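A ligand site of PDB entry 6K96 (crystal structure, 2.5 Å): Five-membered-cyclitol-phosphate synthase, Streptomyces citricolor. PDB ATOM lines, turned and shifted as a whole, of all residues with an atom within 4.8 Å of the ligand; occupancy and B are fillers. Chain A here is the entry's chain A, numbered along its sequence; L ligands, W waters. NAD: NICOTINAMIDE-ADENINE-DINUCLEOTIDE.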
ATOM      1  N   ALA A  10     -12.486  -8.427  12.011  1.00  0.00           N
ATOM      2  CA  ALA A  10     -12.289  -7.394  13.042  1.00  0.00           C
ATOM      3  C   ALA A  10     -13.613  -6.647  13.140  1.00  0.00           C
ATOM      4  O   ALA A  10     -13.898  -5.860  12.318  1.00  0.00           O
ATOM      5  CB  ALA A  10     -11.112  -6.507  12.730  1.00  0.00           C
ATOM      6  N   GLY A  11     -14.414  -6.999  14.110  1.00  0.00           N
ATOM      7  CA  GLY A  11     -15.683  -6.345  14.467  1.00  0.00           C
ATOM      8  C   GLY A  11     -16.808  -7.289  14.170  1.00  0.00           C
ATOM      9  O   GLY A  11     -16.973  -7.651  12.968  1.00  0.00           O
ATOM     10  N   VAL A  12     -17.511  -7.714  15.196  1.00  0.00           N
ATOM     11  CA  VAL A  12     -18.540  -8.776  15.067  1.00  0.00           C
ATOM     12  C   VAL A  12     -19.892  -8.119  15.270  1.00  0.00           C
ATOM     13  O   VAL A  12     -20.629  -8.469  16.202  1.00  0.00           O
ATOM     14  CB  VAL A  12     -18.319  -9.954  16.007  1.00  0.00           C
ATOM     15  CG1 VAL A  12     -19.218 -11.110  15.594  1.00  0.00           C
ATOM     16  CG2 VAL A  12     -16.854 -10.378  15.979  1.00  0.00           C
ATOM     17  N   GLY A  13     -20.211  -7.259  14.308  1.00  0.00           N
ATOM     18  CA  GLY A  13     -21.463  -6.476  14.258  1.00  0.00           C
ATOM     19  C   GLY A  13     -22.473  -7.072  13.338  1.00  0.00           C
ATOM     20  O   GLY A  13     -22.265  -8.211  12.875  1.00  0.00           O
ATOM     21  N   ASN A  14     -23.518  -6.267  13.103  1.00  0.00           N
ATOM     22  CA  ASN A  14     -24.708  -6.572  12.246  1.00  0.00           C
ATOM     23  C   ASN A  14     -24.248  -7.124  10.889  1.00  0.00           C
ATOM     24  O   ASN A  14     -24.689  -8.173  10.528  1.00  0.00           O
ATOM     25  CB  ASN A  14     -25.520  -5.306  12.180  1.00  0.00           C
ATOM     26  CG  ASN A  14     -26.334  -5.121  13.418  1.00  0.00           C
ATOM     27  OD1 ASN A  14     -26.673  -6.108  14.042  1.00  0.00           O
ATOM     28  ND2 ASN A  14     -26.708  -3.872  13.697  1.00  0.00           N
ATOM     29  N   ASN A  15     -23.240  -6.522  10.272  1.00  0.00           N
ATOM     30  CA  ASN A  15     -22.682  -6.942   8.980  1.00  0.00           C
ATOM     31  C   ASN A  15     -22.279  -8.423   9.013  1.00  0.00           C
ATOM     32  O   ASN A  15     -22.533  -9.166   7.916  1.00  0.00           O
ATOM     33  CB  ASN A  15     -21.439  -6.126   8.611  1.00  0.00           C
ATOM     34  CG  ASN A  15     -21.751  -4.694   8.257  1.00  0.00           C
ATOM     35  OD1 ASN A  15     -22.907  -4.298   8.359  1.00  0.00           O
ATOM     36  ND2 ASN A  15     -20.711  -3.946   7.893  1.00  0.00           N
ATOM     37  N   ILE A  16     -21.642  -8.860  10.128  1.00  0.00           N
ATOM     38  CA  ILE A  16     -21.068 -10.226  10.257  1.00  0.00           C
ATOM     39  C   ILE A  16     -22.197 -11.183  10.582  1.00  0.00           C
ATOM     40  O   ILE A  16     -22.161 -12.333  10.148  1.00  0.00           O
ATOM     41  CB  ILE A  16     -19.941 -10.301  11.317  1.00  0.00           C
ATOM     42  CG1 ILE A  16     -18.824  -9.278  11.028  1.00  0.00           C
ATOM     43  CG2 ILE A  16     -19.403 -11.716  11.502  1.00  0.00           C
ATOM     44  CD1 ILE A  16     -18.329  -9.175   9.603  1.00  0.00           C
ATOM     45  N   PHE A  61     -12.191 -10.755  16.220  1.00  0.00           N
ATOM     46  CA  PHE A  61     -11.829  -9.750  17.239  1.00  0.00           C
ATOM     47  C   PHE A  61     -12.975  -8.785  17.501  1.00  0.00           C
ATOM     48  O   PHE A  61     -13.446  -8.121  16.540  1.00  0.00           O
ATOM     49  CB  PHE A  61     -10.569  -9.022  16.798  1.00  0.00           C
ATOM     50  CG  PHE A  61      -9.528  -9.979  16.307  1.00  0.00           C
ATOM     51  CD1 PHE A  61      -9.609 -10.481  15.026  1.00  0.00           C
ATOM     52  CD2 PHE A  61      -8.496 -10.392  17.146  1.00  0.00           C
ATOM     53  CE1 PHE A  61      -8.641 -11.354  14.558  1.00  0.00           C
ATOM     54  CE2 PHE A  61      -7.533 -11.253  16.675  1.00  0.00           C
ATOM     55  CZ  PHE A  61      -7.621 -11.748  15.398  1.00  0.00           C
ATOM     56  N   ASP A  62     -13.340  -8.700  18.791  1.00  0.00           N
ATOM     57  CA  ASP A  62     -14.166  -7.601  19.346  1.00  0.00           C
ATOM     58  C   ASP A  62     -13.588  -7.085  20.680  1.00  0.00           C
ATOM     59  O   ASP A  62     -12.588  -7.587  21.133  1.00  0.00           O
ATOM     60  CB  ASP A  62     -15.606  -8.090  19.468  1.00  0.00           C
ATOM     61  CG  ASP A  62     -16.605  -7.056  18.985  1.00  0.00           C
ATOM     62  OD1 ASP A  62     -16.807  -6.008  19.694  1.00  0.00           O
ATOM     63  OD2 ASP A  62     -17.164  -7.274  17.866  1.00  0.00           O
ATOM     64  N   LEU A  63     -14.282  -6.103  21.267  1.00  0.00           N
ATOM     65  CA  LEU A  63     -14.032  -5.463  22.580  1.00  0.00           C
ATOM     66  C   LEU A  63     -15.263  -5.579  23.484  1.00  0.00           C
ATOM     67  O   LEU A  63     -15.144  -5.223  24.739  1.00  0.00           O
ATOM     68  CB  LEU A  63     -13.713  -3.980  22.371  1.00  0.00           C
ATOM     69  CG  LEU A  63     -12.322  -3.620  21.890  1.00  0.00           C
ATOM     70  CD1 LEU A  63     -12.126  -2.102  21.964  1.00  0.00           C
ATOM     71  CD2 LEU A  63     -11.231  -4.346  22.681  1.00  0.00           C
ATOM     72  N   HIS A  64     -16.430  -5.906  22.906  1.00  0.00           N
ATOM     73  CA  HIS A  64     -17.701  -5.812  23.665  1.00  0.00           C
ATOM     74  C   HIS A  64     -17.823  -7.032  24.565  1.00  0.00           C
ATOM     75  O   HIS A  64     -17.607  -8.150  24.112  1.00  0.00           O
ATOM     76  CB  HIS A  64     -18.903  -5.603  22.755  1.00  0.00           C
ATOM     77  CG  HIS A  64     -20.099  -5.104  23.473  1.00  0.00           C
ATOM     78  ND1 HIS A  64     -20.871  -5.950  24.241  1.00  0.00           N
ATOM     79  CD2 HIS A  64     -20.595  -3.838  23.631  1.00  0.00           C
ATOM     80  CE1 HIS A  64     -21.857  -5.255  24.782  1.00  0.00           C
ATOM     81  NE2 HIS A  64     -21.687  -3.940  24.441  1.00  0.00           N
ATOM     82  N   LYS A  67     -19.466 -10.299  23.546  1.00  0.00           N
ATOM     83  CA  LYS A  67     -18.842 -10.934  22.357  1.00  0.00           C
ATOM     84  C   LYS A  67     -17.430 -11.462  22.662  1.00  0.00           C
ATOM     85  O   LYS A  67     -17.081 -12.493  22.073  1.00  0.00           O
ATOM     86  CB  LYS A  67     -18.806  -9.945  21.173  1.00  0.00           C
ATOM     87  CG  LYS A  67     -20.104  -9.188  20.948  1.00  0.00           C
ATOM     88  CD  LYS A  67     -20.289  -8.710  19.487  1.00  0.00           C
ATOM     89  CE  LYS A  67     -21.562  -7.928  19.221  1.00  0.00           C
ATOM     90  NZ  LYS A  67     -21.316  -6.924  18.172  1.00  0.00           N
ATOM     91  N   ASN A  81     -26.336  -6.443  18.576  1.00  0.00           N
ATOM     92  CA  ASN A  81     -26.644  -6.935  17.196  1.00  0.00           C
ATOM     93  C   ASN A  81     -28.145  -7.210  17.098  1.00  0.00           C
ATOM     94  O   ASN A  81     -28.722  -7.824  18.018  1.00  0.00           O
ATOM     95  CB  ASN A  81     -25.880  -8.211  16.807  1.00  0.00           C
ATOM     96  CG  ASN A  81     -24.391  -7.985  16.598  1.00  0.00           C
ATOM     97  OD1 ASN A  81     -23.878  -6.907  16.848  1.00  0.00           O
ATOM     98  ND2 ASN A  81     -23.705  -9.008  16.159  1.00  0.00           N
ATOM     99  N   GLY A 100     -10.045  -7.619  20.791  1.00  0.00           N
ATOM    100  CA  GLY A 100      -9.531  -6.704  19.755  1.00  0.00           C
ATOM    101  C   GLY A 100      -8.392  -5.824  20.271  1.00  0.00           C
ATOM    102  O   GLY A 100      -8.020  -6.031  21.405  1.00  0.00           O
ATOM    103  N   LEU A 101      -7.833  -4.971  19.405  1.00  0.00           N
ATOM    104  CA  LEU A 101      -6.940  -3.857  19.741  1.00  0.00           C
ATOM    105  C   LEU A 101      -7.729  -2.697  20.327  1.00  0.00           C
ATOM    106  O   LEU A 101      -8.595  -2.176  19.560  1.00  0.00           O
ATOM    107  CB  LEU A 101      -6.285  -3.299  18.487  1.00  0.00           C
ATOM    108  CG  LEU A 101      -5.365  -4.213  17.710  1.00  0.00           C
ATOM    109  CD1 LEU A 101      -5.114  -3.565  16.346  1.00  0.00           C
ATOM    110  CD2 LEU A 101      -4.065  -4.511  18.495  1.00  0.00           C
ATOM    111  N   SER A 131     -14.553  -4.508  10.029  1.00  0.00           N
ATOM    112  CA  SER A 131     -15.993  -4.234  10.113  1.00  0.00           C
ATOM    113  C   SER A 131     -16.291  -3.417  11.411  1.00  0.00           C
ATOM    114  O   SER A 131     -17.377  -3.558  12.033  1.00  0.00           O
ATOM    115  CB  SER A 131     -16.718  -5.565   9.966  1.00  0.00           C
ATOM    116  OG  SER A 131     -18.130  -5.405   9.760  1.00  0.00           O
ATOM    117  N   LEU A 132     -15.416  -2.477  11.737  1.00  0.00           N
ATOM    118  CA  LEU A 132     -15.542  -1.677  12.992  1.00  0.00           C
ATOM    119  C   LEU A 132     -16.472  -0.509  12.699  1.00  0.00           C
ATOM    120  O   LEU A 132     -16.700  -0.145  11.550  1.00  0.00           O
ATOM    121  CB  LEU A 132     -14.181  -1.153  13.491  1.00  0.00           C
ATOM    122  CG  LEU A 132     -13.364  -2.093  14.393  1.00  0.00           C
ATOM    123  CD1 LEU A 132     -12.973  -3.350  13.621  1.00  0.00           C
ATOM    124  CD2 LEU A 132     -12.091  -1.429  14.957  1.00  0.00           C
ATOM    125  N   PRO A 133     -16.947   0.141  13.784  1.00  0.00           N
ATOM    126  CA  PRO A 133     -17.466   1.496  13.748  1.00  0.00           C
ATOM    127  C   PRO A 133     -16.576   2.455  12.956  1.00  0.00           C
ATOM    128  O   PRO A 133     -15.353   2.371  12.832  1.00  0.00           O
ATOM    129  CB  PRO A 133     -17.485   1.966  15.218  1.00  0.00           C
ATOM    130  CG  PRO A 133     -17.578   0.675  16.022  1.00  0.00           C
ATOM    131  CD  PRO A 133     -16.936  -0.395  15.164  1.00  0.00           C
ATOM    132  N   THR A 134     -17.299   3.335  12.313  1.00  0.00           N
ATOM    133  CA  THR A 134     -16.782   4.359  11.379  1.00  0.00           C
ATOM    134  C   THR A 134     -16.211   5.379  12.325  1.00  0.00           C
ATOM    135  O   THR A 134     -16.816   5.505  13.397  1.00  0.00           O
ATOM    136  CB  THR A 134     -17.932   4.794  10.441  1.00  0.00           C
ATOM    137  OG1 THR A 134     -17.953   3.822   9.392  1.00  0.00           O
ATOM    138  CG2 THR A 134     -17.754   6.192   9.894  1.00  0.00           C
ATOM    139  N   LEU A 136     -12.730   5.332  13.349  1.00  0.00           N
ATOM    140  CA  LEU A 136     -11.517   4.822  14.077  1.00  0.00           C
ATOM    141  C   LEU A 136     -10.377   4.567  13.082  1.00  0.00           C
ATOM    142  O   LEU A 136     -10.107   3.379  12.777  1.00  0.00           O
ATOM    143  CB  LEU A 136     -11.853   3.527  14.821  1.00  0.00           C
ATOM    144  CG  LEU A 136     -13.050   3.555  15.784  1.00  0.00           C
ATOM    145  CD1 LEU A 136     -13.330   2.148  16.336  1.00  0.00           C
ATOM    146  CD2 LEU A 136     -12.861   4.565  16.935  1.00  0.00           C
ATOM    147  N   TRP A 138      -7.178   5.044  13.644  1.00  0.00           N
ATOM    148  CA  TRP A 138      -6.024   4.326  14.283  1.00  0.00           C
ATOM    149  C   TRP A 138      -6.224   2.807  14.103  1.00  0.00           C
ATOM    150  O   TRP A 138      -5.178   2.065  13.944  1.00  0.00           O
ATOM    151  CB  TRP A 138      -5.798   4.708  15.775  1.00  0.00           C
ATOM    152  CG  TRP A 138      -6.956   4.383  16.658  1.00  0.00           C
ATOM    153  CD1 TRP A 138      -7.987   5.211  17.000  1.00  0.00           C
ATOM    154  CD2 TRP A 138      -7.273   3.102  17.214  1.00  0.00           C
ATOM    155  NE1 TRP A 138      -8.916   4.547  17.751  1.00  0.00           N
ATOM    156  CE2 TRP A 138      -8.500   3.240  17.913  1.00  0.00           C
ATOM    157  CE3 TRP A 138      -6.652   1.853  17.184  1.00  0.00           C
ATOM    158  CZ2 TRP A 138      -9.094   2.174  18.589  1.00  0.00           C
ATOM    159  CZ3 TRP A 138      -7.224   0.797  17.861  1.00  0.00           C
ATOM    160  CH2 TRP A 138      -8.434   0.958  18.560  1.00  0.00           C
ATOM    161  N   TYR A 143      -5.157  -2.772  12.351  1.00  0.00           N
ATOM    162  CA  TYR A 143      -5.610  -4.078  11.804  1.00  0.00           C
ATOM    163  C   TYR A 143      -4.978  -4.335  10.438  1.00  0.00           C
ATOM    164  O   TYR A 143      -4.717  -5.493  10.074  1.00  0.00           O
ATOM    165  CB  TYR A 143      -7.129  -4.195  11.749  1.00  0.00           C
ATOM    166  CG  TYR A 143      -7.724  -4.448  13.106  1.00  0.00           C
ATOM    167  CD1 TYR A 143      -7.662  -5.697  13.702  1.00  0.00           C
ATOM    168  CD2 TYR A 143      -8.337  -3.434  13.794  1.00  0.00           C
ATOM    169  CE1 TYR A 143      -8.175  -5.927  14.973  1.00  0.00           C
ATOM    170  CE2 TYR A 143      -8.896  -3.656  15.046  1.00  0.00           C
ATOM    171  CZ  TYR A 143      -8.805  -4.891  15.649  1.00  0.00           C
ATOM    172  OH  TYR A 143      -9.387  -5.116  16.862  1.00  0.00           O
ATOM    173  N   CYS A 157     -14.418  -2.191   4.923  1.00  0.00           N
ATOM    174  CA  CYS A 157     -15.837  -1.755   4.814  1.00  0.00           C
ATOM    175  C   CYS A 157     -16.084  -0.254   5.113  1.00  0.00           C
ATOM    176  O   CYS A 157     -17.280   0.187   4.925  1.00  0.00           O
ATOM    177  CB  CYS A 157     -16.687  -2.459   5.843  1.00  0.00           C
ATOM    178  SG  CYS A 157     -16.745  -4.255   5.662  1.00  0.00           S
ATOM    179  N   THR A 158     -15.129   0.451   5.748  1.00  0.00           N
ATOM    180  CA  THR A 158     -15.410   1.762   6.415  1.00  0.00           C
ATOM    181  C   THR A 158     -14.841   2.892   5.548  1.00  0.00           C
ATOM    182  O   THR A 158     -14.023   2.640   4.670  1.00  0.00           O
ATOM    183  CB  THR A 158     -14.835   1.885   7.852  1.00  0.00           C
ATOM    184  OG1 THR A 158     -13.436   2.186   7.801  1.00  0.00           O
ATOM    185  CG2 THR A 158     -15.048   0.641   8.672  1.00  0.00           C
ATOM    186  N   ASP A 183     -14.561   1.651   1.780  1.00  0.00           N
ATOM    187  CA  ASP A 183     -15.937   2.118   2.086  1.00  0.00           C
ATOM    188  C   ASP A 183     -16.922   1.398   1.190  1.00  0.00           C
ATOM    189  O   ASP A 183     -16.978   1.745   0.028  1.00  0.00           O
ATOM    190  CB  ASP A 183     -16.060   3.628   1.942  1.00  0.00           C
ATOM    191  CG  ASP A 183     -17.236   4.185   2.713  1.00  0.00           C
ATOM    192  OD1 ASP A 183     -17.920   3.403   3.425  1.00  0.00           O
ATOM    193  OD2 ASP A 183     -17.433   5.416   2.608  1.00  0.00           O
ATOM    194  N   LEU A 184     -17.708   0.473   1.767  1.00  0.00           N
ATOM    195  CA  LEU A 184     -18.806  -0.249   1.073  1.00  0.00           C
ATOM    196  C   LEU A 184     -19.770   0.733   0.426  1.00  0.00           C
ATOM    197  O   LEU A 184     -20.202   1.668   1.054  1.00  0.00           O
ATOM    198  CB  LEU A 184     -19.563  -1.105   2.087  1.00  0.00           C
ATOM    199  CG  LEU A 184     -18.776  -2.219   2.752  1.00  0.00           C
ATOM    200  CD1 LEU A 184     -19.728  -3.142   3.506  1.00  0.00           C
ATOM    201  CD2 LEU A 184     -17.936  -3.001   1.766  1.00  0.00           C
ATOM    202  N   SER A 186     -23.532   0.448  -0.480  1.00  0.00           N
ATOM    203  CA  SER A 186     -24.688  -0.444  -0.123  1.00  0.00           C
ATOM    204  C   SER A 186     -25.164  -1.203  -1.374  1.00  0.00           C
ATOM    205  O   SER A 186     -25.183  -0.604  -2.452  1.00  0.00           O
ATOM    206  CB  SER A 186     -25.768   0.362   0.493  1.00  0.00           C
ATOM    207  OG  SER A 186     -25.341   0.882   1.745  1.00  0.00           O
ATOM    208  N   ASN A 219     -29.875   0.905  14.606  1.00  0.00           N
ATOM    209  CA  ASN A 219     -28.803  -0.050  14.927  1.00  0.00           C
ATOM    210  C   ASN A 219     -27.562   0.734  15.415  1.00  0.00           C
ATOM    211  O   ASN A 219     -27.547   1.992  15.355  1.00  0.00           O
ATOM    212  CB  ASN A 219     -28.572  -1.006  13.760  1.00  0.00           C
ATOM    213  CG  ASN A 219     -27.931  -0.400  12.537  1.00  0.00           C
ATOM    214  OD1 ASN A 219     -27.539   0.766  12.489  1.00  0.00           O
ATOM    215  ND2 ASN A 219     -27.734  -1.261  11.550  1.00  0.00           N
ATOM    216  N   GLU A 220     -26.536   0.014  15.823  1.00  0.00           N
ATOM    217  CA  GLU A 220     -25.330   0.632  16.408  1.00  0.00           C
ATOM    218  C   GLU A 220     -24.682   1.505  15.322  1.00  0.00           C
ATOM    219  O   GLU A 220     -24.303   2.645  15.642  1.00  0.00           O
ATOM    220  CB  GLU A 220     -24.467  -0.441  17.078  1.00  0.00           C
ATOM    221  CG  GLU A 220     -24.016  -0.075  18.470  1.00  0.00           C
ATOM    222  CD  GLU A 220     -25.033   0.485  19.453  1.00  0.00           C
ATOM    223  OE1 GLU A 220     -26.149  -0.075  19.534  1.00  0.00           O
ATOM    224  OE2 GLU A 220     -24.675   1.462  20.174  1.00  0.00           O
ATOM    225  N   ASP A 221     -24.639   1.053  14.070  1.00  0.00           N
ATOM    226  CA  ASP A 221     -23.973   1.815  12.974  1.00  0.00           C
ATOM    227  C   ASP A 221     -24.644   3.187  12.912  1.00  0.00           C
ATOM    228  O   ASP A 221     -23.961   4.205  12.925  1.00  0.00           O
ATOM    229  CB  ASP A 221     -24.017   0.982  11.681  1.00  0.00           C
ATOM    230  CG  ASP A 221     -23.527   1.610  10.379  1.00  0.00           C
ATOM    231  OD1 ASP A 221     -22.465   2.316  10.421  1.00  0.00           O
ATOM    232  OD2 ASP A 221     -24.179   1.285   9.269  1.00  0.00           O
ATOM    233  N   LEU A 225     -23.045   6.904  13.505  1.00  0.00           N
ATOM    234  CA  LEU A 225     -22.996   8.016  12.499  1.00  0.00           C
ATOM    235  C   LEU A 225     -23.761   9.254  13.040  1.00  0.00           C
ATOM    236  O   LEU A 225     -23.301  10.380  12.820  1.00  0.00           O
ATOM    237  CB  LEU A 225     -23.579   7.539  11.175  1.00  0.00           C
ATOM    238  CG  LEU A 225     -22.906   6.356  10.487  1.00  0.00           C
ATOM    239  CD1 LEU A 225     -23.676   6.059   9.196  1.00  0.00           C
ATOM    240  CD2 LEU A 225     -21.456   6.633  10.158  1.00  0.00           C
ATOM    241  N   ASP A 292     -30.557  -3.108   6.338  1.00  0.00           N
ATOM    242  CA  ASP A 292     -29.343  -2.265   6.080  1.00  0.00           C
ATOM    243  C   ASP A 292     -28.075  -3.165   5.997  1.00  0.00           C
ATOM    244  O   ASP A 292     -27.289  -3.057   5.075  1.00  0.00           O
ATOM    245  CB  ASP A 292     -29.225  -1.135   7.131  1.00  0.00           C
ATOM    246  CG  ASP A 292     -28.174  -0.083   6.779  1.00  0.00           C
ATOM    247  OD1 ASP A 292     -28.050   0.224   5.598  1.00  0.00           O
ATOM    248  OD2 ASP A 292     -27.486   0.436   7.675  1.00  0.00           O
ATOM    249  N   SER A 293     -27.921  -4.115   6.890  1.00  0.00           N
ATOM    250  CA  SER A 293     -26.736  -4.981   6.938  1.00  0.00           C
ATOM    251  C   SER A 293     -26.801  -6.107   5.876  1.00  0.00           C
ATOM    252  O   SER A 293     -25.722  -6.743   5.677  1.00  0.00           O
ATOM    253  CB  SER A 293     -26.517  -5.523   8.326  1.00  0.00           C
ATOM    254  OG  SER A 293     -26.095  -4.473   9.187  1.00  0.00           O
ATOM    255  N   ASN A 295     -27.542  -4.968   2.922  1.00  0.00           N
ATOM    256  CA  ASN A 295     -26.915  -4.057   1.945  1.00  0.00           C
ATOM    257  C   ASN A 295     -25.394  -4.141   2.114  1.00  0.00           C
ATOM    258  O   ASN A 295     -24.693  -3.855   1.134  1.00  0.00           O
ATOM    259  CB  ASN A 295     -27.421  -2.609   2.025  1.00  0.00           C
ATOM    260  CG  ASN A 295     -28.551  -2.278   1.072  1.00  0.00           C
ATOM    261  OD1 ASN A 295     -28.851  -3.048   0.186  1.00  0.00           O
ATOM    262  ND2 ASN A 295     -29.162  -1.138   1.227  1.00  0.00           N
ATOM    263  N   ALA A 296     -24.888  -4.476   3.300  1.00  0.00           N
ATOM    264  CA  ALA A 296     -23.431  -4.660   3.523  1.00  0.00           C
ATOM    265  C   ALA A 296     -23.017  -6.030   3.008  1.00  0.00           C
ATOM    266  O   ALA A 296     -22.137  -6.087   2.192  1.00  0.00           O
ATOM    267  CB  ALA A 296     -23.028  -4.433   4.977  1.00  0.00           C
HETATM  268  PA  NAD L   1     -21.794  -2.622  14.234  1.00  0.00           P
HETATM  269  O1A NAD L   1     -21.687  -1.296  14.880  1.00  0.00           O
HETATM  270  O2A NAD L   1     -22.943  -3.511  14.551  1.00  0.00           O
HETATM  271  O5B NAD L   1     -20.495  -3.530  14.476  1.00  0.00           O
HETATM  272  C5B NAD L   1     -19.278  -3.005  14.935  1.00  0.00           C
HETATM  273  C4B NAD L   1     -18.574  -4.049  15.754  1.00  0.00           C
HETATM  274  O4B NAD L   1     -17.194  -3.642  15.973  1.00  0.00           O
HETATM  275  C3B NAD L   1     -19.160  -4.298  17.148  1.00  0.00           C
HETATM  276  O3B NAD L   1     -19.085  -5.675  17.493  1.00  0.00           O
HETATM  277  C2B NAD L   1     -18.202  -3.504  18.040  1.00  0.00           C
HETATM  278  O2B NAD L   1     -18.209  -4.021  19.331  1.00  0.00           O
HETATM  279  C1B NAD L   1     -16.907  -3.872  17.340  1.00  0.00           C
HETATM  280  N9A NAD L   1     -15.712  -3.127  17.773  1.00  0.00           N
HETATM  281  C8A NAD L   1     -15.608  -1.818  18.209  1.00  0.00           C
HETATM  282  N7A NAD L   1     -14.370  -1.445  18.394  1.00  0.00           N
HETATM  283  C5A NAD L   1     -13.624  -2.563  18.049  1.00  0.00           C
HETATM  284  C6A NAD L   1     -12.242  -2.824  18.066  1.00  0.00           C
HETATM  285  N6A NAD L   1     -11.363  -1.897  18.394  1.00  0.00           N
HETATM  286  N1A NAD L   1     -11.801  -4.041  17.662  1.00  0.00           N
HETATM  287  C2A NAD L   1     -12.717  -4.935  17.270  1.00  0.00           C
HETATM  288  N3A NAD L   1     -14.051  -4.809  17.228  1.00  0.00           N
HETATM  289  C4A NAD L   1     -14.436  -3.590  17.635  1.00  0.00           C
HETATM  290  O3  NAD L   1     -21.562  -2.286  12.727  1.00  0.00           O
HETATM  291  PN  NAD L   1     -21.960  -2.941  11.341  1.00  0.00           P
HETATM  292  O1N NAD L   1     -21.293  -4.266  11.200  1.00  0.00           O
HETATM  293  O2N NAD L   1     -23.442  -2.834  11.132  1.00  0.00           O
HETATM  294  O5D NAD L   1     -21.202  -1.857  10.480  1.00  0.00           O
HETATM  295  C5D NAD L   1     -19.832  -2.067  10.251  1.00  0.00           C
HETATM  296  C4D NAD L   1     -19.297  -0.945   9.410  1.00  0.00           C
HETATM  297  O4D NAD L   1     -19.824  -1.029   8.057  1.00  0.00           O
HETATM  298  C3D NAD L   1     -19.662   0.459   9.914  1.00  0.00           C
HETATM  299  O3D NAD L   1     -18.457   1.221   9.909  1.00  0.00           O
HETATM  300  C2D NAD L   1     -20.616   0.971   8.846  1.00  0.00           C
HETATM  301  O2D NAD L   1     -20.632   2.378   8.818  1.00  0.00           O
HETATM  302  C1D NAD L   1     -19.984   0.328   7.606  1.00  0.00           C
HETATM  303  N1N NAD L   1     -20.834   0.343   6.355  1.00  0.00           N
HETATM  304  C2N NAD L   1     -21.994  -0.327   6.411  1.00  0.00           C
HETATM  305  C3N NAD L   1     -22.971  -0.157   5.465  1.00  0.00           C
HETATM  306  C7N NAD L   1     -24.066  -1.143   5.740  1.00  0.00           C
HETATM  307  O7N NAD L   1     -24.240  -1.594   6.860  1.00  0.00           O
HETATM  308  N7N NAD L   1     -24.754  -1.545   4.702  1.00  0.00           N
HETATM  309  C4N NAD L   1     -22.787   0.714   4.392  1.00  0.00           C
HETATM  310  C5N NAD L   1     -21.530   1.242   4.183  1.00  0.00           C
HETATM  311  C6N NAD L   1     -20.533   1.031   5.151  1.00  0.00           C
HETATM  312  O   HOH W   1     -20.415   4.298   6.445  1.00  0.00           O
HETATM  313  O   HOH W   2     -20.638  -5.057  19.823  1.00  0.00           O
HETATM  314  O   HOH W   3     -11.805   0.898  19.873  1.00  0.00           O
HETATM  315  O   HOH W   4     -20.916   1.203  14.466  1.00  0.00           O
HETATM  316  O   HOH W   5     -20.193   2.640  12.499  1.00  0.00           O
HETATM  317  O   HOH W   6     -23.553   3.333   7.387  1.00  0.00           O
HETATM  318  O   HOH W   7     -25.070  -1.883  13.274  1.00  0.00           O
HETATM  319  O   HOH W   8     -24.590  -4.118  17.130  1.00  0.00           O
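The backbone carbonyl oxygen of Phe 61 lies close to a nitrogen (N3A) of the ligand (3.4 Å).
The backbone NH (N) of Ala 296 sits close to a nitrogen (N7N) of the ligand (3.3 Å).
Residues that only touch the ligand: Gly 13 (3.1 Å), Pro 133 (3.4 Å), Cys 157 (3.4 Å), Ser 131 (3.4 Å), Leu 184 (3.4 Å), Gly 11 (3.4 Å), Glu 220 (3.6 Å), Leu 63 (3.7 Å), Thr 158 (3.7 Å), Ser 293 (3.7 Å), Ser 186 (3.7 Å), Asn 295 (3.7 Å), His 64 (3.8 Å) and Asp 183 (3.9 Å).
The backbone NH of Ser 131 sits at hydrogen-bond distance from the backbone carbonyl oxygen of Ala 10 (2.7 Å).
N of Gly 11 sits at hydrogen-bond distance from O of Phe 61.
O of Thr 158 sits at hydrogen-bond distance from N of Asp 183 (3.1 Å).
The side-chain hydroxyl (OH) of Tyr 143 sits at hydrogen-bond distance from the backbone NH (N) of Leu 101, at 3.0 Å.
The side-chain amide nitrogen of Asn 81 is in hydrogen-bond range of the backbone carbonyl oxygen of Val 12, 3.1 Å away.
O of Val 12 lies within hydrogen-bond range of NZ of Lys 67, 2.6 Å away.
The backbone NH (N) of Asp 221 lies close to the side-chain amide oxygen (OD1) of Asn 219, 3.3 Å away.
The side-chain amino group (NZ) of Lys 67 sits at hydrogen-bond distance from the side-chain amide oxygen (OD1) of Asn 81 (2.9 Å).
Water W2 bridges NZ of Lys 67 (2.6 Å) and O2B of the ligand (2.7 Å).
Water W8 bridges the side-chain amide oxygen of Asn 81 and an oxygen (O2A) of the ligand.
Water W6 bridges OD2 of Asp 221 (2.9 Å) and O2D of the ligand (3.4 Å).
Water W5 lies within hydrogen-bond range of N of Thr 134 (3.0 Å), OD1 of Asp 221 (3.1 Å) and O3D of the ligand (3.4 Å).
N1A of the ligand sits at hydrogen-bond distance from OH of Tyr 143 (2.8 Å).
N of Val 12 lies close to O3B of the ligand, 3.5 Å away.
N6A of the ligand lies within hydrogen-bond range of O of Leu 101 (3.0 Å).
ND2 of Asn 15 sits at hydrogen-bond distance from O4D of the ligand (3.1 Å).
An oxygen (O1N) of the ligand sits close to the backbone NH (N) of Asn 15.
The side-chain hydroxyl of Thr 134 sits at hydrogen-bond distance from an oxygen (O3D) of the ligand (2.7 Å).
A nitrogen (N7N) of the ligand lies within hydrogen-bond range of the backbone carbonyl oxygen of Asp 292.
The side-chain carboxylate of Asp 62 lies within hydrogen-bond range of an oxygen (O2B) of the ligand (2.5 Å).
The backbone carbonyl oxygen (O) of Val 12 lies close to an oxygen (O3B) of the ligand, 3.4 Å away.
The backbone NH of Thr 134 sits at hydrogen-bond distance from an oxygen (O3D) of the ligand (3.4 Å).
The side-chain carboxylate of Asp 221 sits at hydrogen-bond distance from an oxygen (O2D) of the ligand, at 2.4 Å.
The backbone NH of Asn 14 lies within hydrogen-bond range of an oxygen (O2A) of the ligand, at 3.2 Å.
NZ of Lys 67 is in hydrogen-bond range of O3B of the ligand, 2.6 Å away.
An oxygen (O3D) of the ligand sits at hydrogen-bond distance from the backbone carbonyl oxygen (O) of Leu 132 (2.8 Å).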
